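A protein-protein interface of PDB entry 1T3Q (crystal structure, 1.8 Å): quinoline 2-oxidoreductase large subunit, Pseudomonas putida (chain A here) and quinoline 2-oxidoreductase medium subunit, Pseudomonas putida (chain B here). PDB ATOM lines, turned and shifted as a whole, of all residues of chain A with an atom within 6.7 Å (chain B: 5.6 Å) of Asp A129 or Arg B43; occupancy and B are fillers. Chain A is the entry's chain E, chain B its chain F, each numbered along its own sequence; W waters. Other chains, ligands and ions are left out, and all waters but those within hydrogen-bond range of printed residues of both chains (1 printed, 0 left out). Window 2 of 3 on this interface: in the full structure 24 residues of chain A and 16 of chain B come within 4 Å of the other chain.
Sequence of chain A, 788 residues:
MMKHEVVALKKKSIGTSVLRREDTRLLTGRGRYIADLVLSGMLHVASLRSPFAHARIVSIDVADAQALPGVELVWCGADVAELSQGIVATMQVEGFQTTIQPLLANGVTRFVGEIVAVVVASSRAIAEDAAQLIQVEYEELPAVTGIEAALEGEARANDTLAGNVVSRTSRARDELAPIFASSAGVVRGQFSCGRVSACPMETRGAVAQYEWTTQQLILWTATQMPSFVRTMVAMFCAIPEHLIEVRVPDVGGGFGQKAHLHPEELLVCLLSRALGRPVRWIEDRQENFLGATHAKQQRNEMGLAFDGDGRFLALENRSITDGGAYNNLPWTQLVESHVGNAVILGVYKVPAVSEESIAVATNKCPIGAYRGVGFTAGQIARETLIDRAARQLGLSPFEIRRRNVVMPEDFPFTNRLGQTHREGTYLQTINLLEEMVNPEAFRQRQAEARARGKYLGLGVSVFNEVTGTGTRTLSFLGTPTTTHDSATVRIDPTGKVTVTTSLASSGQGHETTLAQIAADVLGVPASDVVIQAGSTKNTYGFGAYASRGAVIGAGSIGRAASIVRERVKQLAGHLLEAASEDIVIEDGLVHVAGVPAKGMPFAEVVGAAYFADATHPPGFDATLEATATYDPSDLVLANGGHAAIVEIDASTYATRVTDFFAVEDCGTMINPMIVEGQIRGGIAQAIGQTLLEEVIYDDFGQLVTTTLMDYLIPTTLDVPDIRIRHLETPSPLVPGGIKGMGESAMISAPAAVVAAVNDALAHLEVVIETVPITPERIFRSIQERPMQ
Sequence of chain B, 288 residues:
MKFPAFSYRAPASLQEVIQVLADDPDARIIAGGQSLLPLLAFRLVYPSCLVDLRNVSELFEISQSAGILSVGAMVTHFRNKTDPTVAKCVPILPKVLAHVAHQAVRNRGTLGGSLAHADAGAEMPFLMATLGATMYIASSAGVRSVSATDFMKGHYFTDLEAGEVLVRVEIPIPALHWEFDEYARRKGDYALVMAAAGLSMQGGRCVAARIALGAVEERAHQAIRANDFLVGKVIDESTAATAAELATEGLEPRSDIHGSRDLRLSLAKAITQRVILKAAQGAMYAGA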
ATOM      1  N   ALA A  46      14.951  -4.977  20.704  1.00  0.00           N
ATOM      2  CA  ALA A  46      14.946  -3.838  19.796  1.00  0.00           C
ATOM      3  C   ALA A  46      14.348  -4.387  18.505  1.00  0.00           C
ATOM      4  O   ALA A  46      14.489  -5.576  18.216  1.00  0.00           O
ATOM      5  CB  ALA A  46      16.366  -3.322  19.554  1.00  0.00           C
ATOM      6  N   ALA A  65      24.145  -9.657  12.723  1.00  0.00           N
ATOM      7  CA  ALA A  65      23.431  -9.228  13.921  1.00  0.00           C
ATOM      8  C   ALA A  65      23.542 -10.290  15.010  1.00  0.00           C
ATOM      9  O   ALA A  65      23.772  -9.973  16.173  1.00  0.00           O
ATOM     10  CB  ALA A  65      21.970  -8.972  13.594  1.00  0.00           C
ATOM     11  N   LEU A  68      27.093 -10.309  16.728  1.00  0.00           N
ATOM     12  CA  LEU A  68      27.542  -9.166  17.511  1.00  0.00           C
ATOM     13  C   LEU A  68      27.562  -9.537  18.993  1.00  0.00           C
ATOM     14  O   LEU A  68      26.606 -10.116  19.511  1.00  0.00           O
ATOM     15  CB  LEU A  68      26.613  -7.976  17.286  1.00  0.00           C
ATOM     16  CG  LEU A  68      27.065  -6.643  17.890  1.00  0.00           C
ATOM     17  CD1 LEU A  68      28.279  -6.117  17.114  1.00  0.00           C
ATOM     18  CD2 LEU A  68      25.921  -5.640  17.822  1.00  0.00           C
ATOM     19  N   VAL A  71      24.493  -9.900  21.835  1.00  0.00           N
ATOM     20  CA  VAL A  71      23.247 -10.349  21.217  1.00  0.00           C
ATOM     21  C   VAL A  71      22.988 -11.810  21.575  1.00  0.00           C
ATOM     22  O   VAL A  71      23.873 -12.658  21.437  1.00  0.00           O
ATOM     23  CB  VAL A  71      23.301 -10.215  19.676  1.00  0.00           C
ATOM     24  CG1 VAL A  71      22.010 -10.746  19.055  1.00  0.00           C
ATOM     25  CG2 VAL A  71      23.507  -8.759  19.292  1.00  0.00           C
ATOM     26  N   SER A 123      21.681  -5.171  26.300  1.00  0.00           N
ATOM     27  CA  SER A 123      21.224  -3.805  26.553  1.00  0.00           C
ATOM     28  C   SER A 123      20.404  -3.345  25.362  1.00  0.00           C
ATOM     29  O   SER A 123      20.505  -3.913  24.271  1.00  0.00           O
ATOM     30  CB  SER A 123      22.409  -2.844  26.759  1.00  0.00           C
ATOM     31  OG  SER A 123      23.041  -2.521  25.529  1.00  0.00           O
ATOM     32  N   ARG A 124      19.581  -2.324  25.569  1.00  0.00           N
ATOM     33  CA  ARG A 124      18.763  -1.794  24.491  1.00  0.00           C
ATOM     34  C   ARG A 124      19.650  -1.188  23.391  1.00  0.00           C
ATOM     35  O   ARG A 124      19.368  -1.346  22.203  1.00  0.00           O
ATOM     36  CB  ARG A 124      17.800  -0.741  25.055  1.00  0.00           C
ATOM     37  CG  ARG A 124      17.096   0.111  24.017  1.00  0.00           C
ATOM     38  CD  ARG A 124      16.164  -0.676  23.104  1.00  0.00           C
ATOM     39  NE  ARG A 124      15.525   0.245  22.164  1.00  0.00           N
ATOM     40  CZ  ARG A 124      14.227   0.262  21.878  1.00  0.00           C
ATOM     41  NH1 ARG A 124      13.399  -0.603  22.450  1.00  0.00           N
ATOM     42  NH2 ARG A 124      13.752   1.179  21.040  1.00  0.00           N
ATOM     43  N   ALA A 125      20.721  -0.503  23.791  1.00  0.00           N
ATOM     44  CA  ALA A 125      21.629   0.124  22.834  1.00  0.00           C
ATOM     45  C   ALA A 125      22.278  -0.912  21.922  1.00  0.00           C
ATOM     46  O   ALA A 125      22.330  -0.733  20.705  1.00  0.00           O
ATOM     47  CB  ALA A 125      22.708   0.927  23.568  1.00  0.00           C
ATOM     48  N   ILE A 126      22.774  -1.993  22.513  1.00  0.00           N
ATOM     49  CA  ILE A 126      23.407  -3.051  21.735  1.00  0.00           C
ATOM     50  C   ILE A 126      22.376  -3.774  20.864  1.00  0.00           C
ATOM     51  O   ILE A 126      22.688  -4.208  19.752  1.00  0.00           O
ATOM     52  CB  ILE A 126      24.128  -4.061  22.660  1.00  0.00           C
ATOM     53  CG1 ILE A 126      25.313  -3.368  23.341  1.00  0.00           C
ATOM     54  CG2 ILE A 126      24.594  -5.278  21.859  1.00  0.00           C
ATOM     55  CD1 ILE A 126      25.971  -4.203  24.434  1.00  0.00           C
ATOM     56  N   ALA A 127      21.149  -3.902  21.360  1.00  0.00           N
ATOM     57  CA  ALA A 127      20.108  -4.546  20.572  1.00  0.00           C
ATOM     58  C   ALA A 127      19.884  -3.697  19.317  1.00  0.00           C
ATOM     59  O   ALA A 127      19.685  -4.226  18.220  1.00  0.00           O
ATOM     60  CB  ALA A 127      18.818  -4.656  21.384  1.00  0.00           C
ATOM     61  N   GLU A 128      19.928  -2.375  19.479  1.00  0.00           N
ATOM     62  CA  GLU A 128      19.750  -1.476  18.345  1.00  0.00           C
ATOM     63  C   GLU A 128      20.960  -1.561  17.407  1.00  0.00           C
ATOM     64  O   GLU A 128      20.801  -1.494  16.187  1.00  0.00           O
ATOM     65  CB  GLU A 128      19.538  -0.030  18.820  1.00  0.00           C
ATOM     66  CG  GLU A 128      18.215   0.171  19.549  1.00  0.00           C
ATOM     67  CD  GLU A 128      17.925   1.616  19.920  1.00  0.00           C
ATOM     68  OE1 GLU A 128      16.845   1.858  20.495  1.00  0.00           O
ATOM     69  OE2 GLU A 128      18.757   2.511  19.647  1.00  0.00           O
ATOM     70  N   ASP A 129      22.158  -1.711  17.975  1.00  0.00           N
ATOM     71  CA  ASP A 129      23.379  -1.835  17.168  1.00  0.00           C
ATOM     72  C   ASP A 129      23.236  -3.034  16.225  1.00  0.00           C
ATOM     73  O   ASP A 129      23.579  -2.958  15.041  1.00  0.00           O
ATOM     74  CB  ASP A 129      24.620  -2.072  18.046  1.00  0.00           C
ATOM     75  CG  ASP A 129      25.014  -0.858  18.883  1.00  0.00           C
ATOM     76  OD1 ASP A 129      24.629   0.275  18.534  1.00  0.00           O
ATOM     77  OD2 ASP A 129      25.738  -1.043  19.889  1.00  0.00           O
ATOM     78  N   ALA A 130      22.740  -4.146  16.762  1.00  0.00           N
ATOM     79  CA  ALA A 130      22.568  -5.363  15.974  1.00  0.00           C
ATOM     80  C   ALA A 130      21.479  -5.207  14.916  1.00  0.00           C
ATOM     81  O   ALA A 130      21.633  -5.666  13.783  1.00  0.00           O
ATOM     82  CB  ALA A 130      22.245  -6.547  16.896  1.00  0.00           C
ATOM     83  N   ALA A 131      20.380  -4.559  15.287  1.00  0.00           N
ATOM     84  CA  ALA A 131      19.275  -4.345  14.357  1.00  0.00           C
ATOM     85  C   ALA A 131      19.745  -3.638  13.085  1.00  0.00           C
ATOM     86  O   ALA A 131      19.258  -3.927  11.987  1.00  0.00           O
ATOM     87  CB  ALA A 131      18.174  -3.533  15.032  1.00  0.00           C
ATOM     88  N   GLN A 132      20.690  -2.714  13.230  1.00  0.00           N
ATOM     89  CA  GLN A 132      21.208  -1.982  12.078  1.00  0.00           C
ATOM     90  C   GLN A 132      22.112  -2.846  11.207  1.00  0.00           C
ATOM     91  O   GLN A 132      22.502  -2.437  10.112  1.00  0.00           O
ATOM     92  CB  GLN A 132      21.991  -0.749  12.523  1.00  0.00           C
ATOM     93  CG  GLN A 132      21.221   0.188  13.421  1.00  0.00           C
ATOM     94  CD  GLN A 132      21.786   1.589  13.389  1.00  0.00           C
ATOM     95  OE1 GLN A 132      21.428   2.391  12.525  1.00  0.00           O
ATOM     96  NE2 GLN A 132      22.690   1.887  14.317  1.00  0.00           N
ATOM     97  N   LEU A 133      22.465  -4.027  11.699  1.00  0.00           N
ATOM     98  CA  LEU A 133      23.321  -4.934  10.939  1.00  0.00           C
ATOM     99  C   LEU A 133      22.468  -5.881  10.101  1.00  0.00           C
ATOM    100  O   LEU A 133      22.973  -6.559   9.207  1.00  0.00           O
ATOM    101  CB  LEU A 133      24.214  -5.745  11.883  1.00  0.00           C
ATOM    102  CG  LEU A 133      25.190  -4.938  12.745  1.00  0.00           C
ATOM    103  CD1 LEU A 133      26.032  -5.880  13.590  1.00  0.00           C
ATOM    104  CD2 LEU A 133      26.077  -4.087  11.847  1.00  0.00           C
ATOM    105  N   ILE A 134      21.173  -5.933  10.403  1.00  0.00           N
ATOM    106  CA  ILE A 134      20.257  -6.798   9.672  1.00  0.00           C
ATOM    107  C   ILE A 134      20.025  -6.246   8.268  1.00  0.00           C
ATOM    108  O   ILE A 134      19.770  -5.054   8.096  1.00  0.00           O
ATOM    109  CB  ILE A 134      18.896  -6.917  10.397  1.00  0.00           C
ATOM    110  CG1 ILE A 134      19.098  -7.526  11.786  1.00  0.00           C
ATOM    111  CG2 ILE A 134      17.939  -7.779   9.579  1.00  0.00           C
ATOM    112  CD1 ILE A 134      17.828  -7.625  12.609  1.00  0.00           C
ATOM    113  N   LYS B   2      18.686   4.999  21.199  1.00  0.00           N
ATOM    114  CA  LYS B   2      19.927   5.149  21.954  1.00  0.00           C
ATOM    115  C   LYS B   2      21.044   5.604  21.026  1.00  0.00           C
ATOM    116  O   LYS B   2      21.084   5.216  19.850  1.00  0.00           O
ATOM    117  CB  LYS B   2      20.319   3.828  22.628  1.00  0.00           C
ATOM    118  CG  LYS B   2      19.249   3.250  23.563  1.00  0.00           C
ATOM    119  CD  LYS B   2      18.827   4.253  24.638  1.00  0.00           C
ATOM    120  CE  LYS B   2      17.744   3.668  25.544  1.00  0.00           C
ATOM    121  NZ  LYS B   2      17.183   4.673  26.495  1.00  0.00           N
ATOM    122  N   PHE B   3      21.943   6.434  21.548  1.00  0.00           N
ATOM    123  CA  PHE B   3      23.068   6.935  20.760  1.00  0.00           C
ATOM    124  C   PHE B   3      23.961   5.788  20.326  1.00  0.00           C
ATOM    125  O   PHE B   3      24.062   4.772  21.008  1.00  0.00           O
ATOM    126  CB  PHE B   3      23.970   7.857  21.584  1.00  0.00           C
ATOM    127  CG  PHE B   3      23.254   8.959  22.303  1.00  0.00           C
ATOM    128  CD1 PHE B   3      23.754   9.433  23.514  1.00  0.00           C
ATOM    129  CD2 PHE B   3      22.111   9.537  21.776  1.00  0.00           C
ATOM    130  CE1 PHE B   3      23.121  10.469  24.191  1.00  0.00           C
ATOM    131  CE2 PHE B   3      21.468  10.575  22.445  1.00  0.00           C
ATOM    132  CZ  PHE B   3      21.976  11.040  23.657  1.00  0.00           C
ATOM    133  N   PRO B   4      24.620   5.933  19.173  1.00  0.00           N
ATOM    134  CA  PRO B   4      25.512   4.854  18.745  1.00  0.00           C
ATOM    135  C   PRO B   4      26.732   4.977  19.669  1.00  0.00           C
ATOM    136  O   PRO B   4      26.868   5.975  20.387  1.00  0.00           O
ATOM    137  CB  PRO B   4      25.822   5.213  17.291  1.00  0.00           C
ATOM    138  CG  PRO B   4      25.667   6.713  17.254  1.00  0.00           C
ATOM    139  CD  PRO B   4      24.451   6.949  18.119  1.00  0.00           C
ATOM    140  N   ALA B   5      27.610   3.980  19.670  1.00  0.00           N
ATOM    141  CA  ALA B   5      28.783   4.029  20.533  1.00  0.00           C
ATOM    142  C   ALA B   5      29.848   5.010  20.044  1.00  0.00           C
ATOM    143  O   ALA B   5      30.002   5.237  18.846  1.00  0.00           O
ATOM    144  CB  ALA B   5      29.383   2.634  20.675  1.00  0.00           C
ATOM    145  N   PRO B  38      20.155  14.947  19.760  1.00  0.00           N
ATOM    146  CA  PRO B  38      18.923  14.485  19.110  1.00  0.00           C
ATOM    147  C   PRO B  38      19.270  13.738  17.818  1.00  0.00           C
ATOM    148  O   PRO B  38      18.634  12.744  17.478  1.00  0.00           O
ATOM    149  CB  PRO B  38      18.162  15.782  18.863  1.00  0.00           C
ATOM    150  CG  PRO B  38      18.516  16.586  20.081  1.00  0.00           C
ATOM    151  CD  PRO B  38      20.022  16.351  20.192  1.00  0.00           C
ATOM    152  N   LEU B  39      20.288  14.216  17.107  1.00  0.00           N
ATOM    153  CA  LEU B  39      20.731  13.564  15.873  1.00  0.00           C
ATOM    154  C   LEU B  39      21.313  12.186  16.183  1.00  0.00           C
ATOM    155  O   LEU B  39      21.120  11.226  15.425  1.00  0.00           O
ATOM    156  CB  LEU B  39      21.795  14.414  15.163  1.00  0.00           C
ATOM    157  CG  LEU B  39      21.343  15.743  14.554  1.00  0.00           C
ATOM    158  CD1 LEU B  39      22.528  16.423  13.872  1.00  0.00           C
ATOM    159  CD2 LEU B  39      20.230  15.490  13.553  1.00  0.00           C
ATOM    160  N   LEU B  40      22.039  12.091  17.291  1.00  0.00           N
ATOM    161  CA  LEU B  40      22.626  10.815  17.700  1.00  0.00           C
ATOM    162  C   LEU B  40      21.521   9.848  18.101  1.00  0.00           C
ATOM    163  O   LEU B  40      21.607   8.651  17.834  1.00  0.00           O
ATOM    164  CB  LEU B  40      23.582  10.998  18.883  1.00  0.00           C
ATOM    165  CG  LEU B  40      24.968  11.563  18.584  1.00  0.00           C
ATOM    166  CD1 LEU B  40      25.758  11.698  19.882  1.00  0.00           C
ATOM    167  CD2 LEU B  40      25.690  10.631  17.619  1.00  0.00           C
ATOM    168  N   ALA B  41      20.488  10.376  18.750  1.00  0.00           N
ATOM    169  CA  ALA B  41      19.367   9.558  19.195  1.00  0.00           C
ATOM    170  C   ALA B  41      18.701   8.880  18.002  1.00  0.00           C
ATOM    171  O   ALA B  41      18.214   7.756  18.112  1.00  0.00           O
ATOM    172  CB  ALA B  41      18.358  10.425  19.944  1.00  0.00           C
ATOM    173  N   PHE B  42      18.684   9.573  16.866  1.00  0.00           N
ATOM    174  CA  PHE B  42      18.091   9.052  15.636  1.00  0.00           C
ATOM    175  C   PHE B  42      19.124   8.294  14.815  1.00  0.00           C
ATOM    176  O   PHE B  42      18.812   7.753  13.753  1.00  0.00           O
ATOM    177  CB  PHE B  42      17.535  10.199  14.792  1.00  0.00           C
ATOM    178  CG  PHE B  42      16.275  10.800  15.335  1.00  0.00           C
ATOM    179  CD1 PHE B  42      16.025  12.160  15.204  1.00  0.00           C
ATOM    180  CD2 PHE B  42      15.321  10.001  15.949  1.00  0.00           C
ATOM    181  CE1 PHE B  42      14.841  12.716  15.680  1.00  0.00           C
ATOM    182  CE2 PHE B  42      14.141  10.544  16.423  1.00  0.00           C
ATOM    183  CZ  PHE B  42      13.895  11.902  16.291  1.00  0.00           C
ATOM    184  N   ARG B  43      20.355   8.260  15.314  1.00  0.00           N
ATOM    185  CA  ARG B  43      21.452   7.593  14.626  1.00  0.00           C
ATOM    186  C   ARG B  43      21.613   8.128  13.206  1.00  0.00           C
ATOM    187  O   ARG B  43      21.745   7.369  12.245  1.00  0.00           O
ATOM    188  CB  ARG B  43      21.230   6.079  14.625  1.00  0.00           C
ATOM    189  CG  ARG B  43      21.120   5.522  16.041  1.00  0.00           C
ATOM    190  CD  ARG B  43      21.495   4.061  16.136  1.00  0.00           C
ATOM    191  NE  ARG B  43      21.545   3.633  17.532  1.00  0.00           N
ATOM    192  CZ  ARG B  43      22.201   2.559  17.959  1.00  0.00           C
ATOM    193  NH1 ARG B  43      22.868   1.798  17.099  1.00  0.00           N
ATOM    194  NH2 ARG B  43      22.194   2.248  19.249  1.00  0.00           N
ATOM    195  N   LEU B  44      21.603   9.452  13.092  1.00  0.00           N
ATOM    196  CA  LEU B  44      21.770  10.115  11.806  1.00  0.00           C
ATOM    197  C   LEU B  44      23.249  10.426  11.578  1.00  0.00           C
ATOM    198  O   LEU B  44      23.659  10.739  10.463  1.00  0.00           O
ATOM    199  CB  LEU B  44      20.948  11.407  11.757  1.00  0.00           C
ATOM    200  CG  LEU B  44      19.434  11.239  11.896  1.00  0.00           C
ATOM    201  CD1 LEU B  44      18.763  12.598  11.782  1.00  0.00           C
ATOM    202  CD2 LEU B  44      18.912  10.290  10.815  1.00  0.00           C
ATOM    203  N   VAL B  45      24.038  10.340  12.646  1.00  0.00           N
ATOM    204  CA  VAL B  45      25.481  10.584  12.579  1.00  0.00           C
ATOM    205  C   VAL B  45      26.176   9.528  13.436  1.00  0.00           C
ATOM    206  O   VAL B  45      25.637   9.098  14.459  1.00  0.00           O
ATOM    207  CB  VAL B  45      25.864  12.002  13.093  1.00  0.00           C
ATOM    208  CG1 VAL B  45      25.187  13.065  12.238  1.00  0.00           C
ATOM    209  CG2 VAL B  45      25.469  12.166  14.543  1.00  0.00           C
ATOM    210  N   TYR B  46      27.361   9.103  13.012  1.00  0.00           N
ATOM    211  CA  TYR B  46      28.107   8.084  13.740  1.00  0.00           C
ATOM    212  C   TYR B  46      29.534   8.521  14.036  1.00  0.00           C
ATOM    213  O   TYR B  46      30.481   8.068  13.397  1.00  0.00           O
ATOM    214  CB  TYR B  46      28.126   6.776  12.947  1.00  0.00           C
ATOM    215  CG  TYR B  46      26.751   6.215  12.668  1.00  0.00           C
ATOM    216  CD1 TYR B  46      25.926   6.785  11.697  1.00  0.00           C
ATOM    217  CD2 TYR B  46      26.261   5.129  13.392  1.00  0.00           C
ATOM    218  CE1 TYR B  46      24.649   6.289  11.455  1.00  0.00           C
ATOM    219  CE2 TYR B  46      24.983   4.623  13.156  1.00  0.00           C
ATOM    220  CZ  TYR B  46      24.184   5.209  12.189  1.00  0.00           C
ATOM    221  OH  TYR B  46      22.920   4.715  11.954  1.00  0.00           O
HETATM  222  O   HOH W   1      26.995   1.766  18.048  1.00  0.00           O
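The side-chain carboxylate (OE2) of Glu A128 lies within hydrogen-bond range of the backbone NH (N) of Lys B2 (2.9 Å). NH2 of Arg B43 sits at hydrogen-bond distance from O of Ala A125 (3.3 Å). OD1 of Asp A129 lies within salt-bridge range of NH1 of Arg B43 (2.7 Å). NH1 of Arg B43 sits close to NE2 of Gln A132. OE1 of Gln A132 lies within hydrogen-bond range of OH of Tyr B46. The side-chain carboxylate of Glu A128 lies within salt-bridge range of the guanidinium group of Arg B43 (3.5 Å).
O of Arg B43 is in hydrogen-bond range of OH of Tyr B46, 2.9 Å away. The guanidinium group (NE) of Arg A124 is in salt-bridge range of the side-chain carboxylate (OE1) of Glu A128 (2.7 Å). The backbone carbonyl oxygen (O) of Lys B2 is in hydrogen-bond range of the guanidinium group (NE) of Arg B43, at 2.8 Å.
Among the printed residues, merely in contact across the chains: Arg A124 with Lys B2 (3.8 Å) and Ala A125 with Lys B2 (3.9 Å).
Val A71 touches none of the printed residues of chain B. Of the printed residues of chain B, Ala A125 touches Lys B2 (3.9 Å) and Arg B43 (3.3 Å). Printed residues of chain B within 4 Å of Glu A128: Lys B2 and Arg B43. Of chain B, only Arg B43 (2.7 Å) comes within 4 Å of Asp A129. Printed residues of chain B within 4 Å of Gln A132: Arg B43 (2.8 Å) and Tyr B46 (2.8 Å). Printed residues of chain A within 4 Å of Lys B2: Arg A124 (3.8 Å), Ala A125 (3.9 Å) and Glu A128 (2.9 Å). Arg B43 touches just these residues of chain A: Ala A125, Glu A128, Asp A129 and Gln A132. Leu B44 touches none of the printed residues of chain A. Printed residues of chain A within 4 Å of Tyr B46: Gln A132. The nearest residue of chain B that does not touch Asp A129 is Pro B4 (4.7 Å). The nearest residue of chain A that does not touch Arg B43 is Ile A126 (5.4 Å).
Of the 13 printed residues of chain B, 3 touch a printed residue of chain A. Along chain B the printed residues that touch a printed residue of chain A span positions 2 to 46. Hydrophobic or aromatic side chains of chain A that line the printed part of chain B: Ala A125.
Water W1 bridges the backbone NH (N) of Ala B5 (2.8 Å) and the side-chain carboxylate (OD1) of Asp A129 (2.8 Å).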
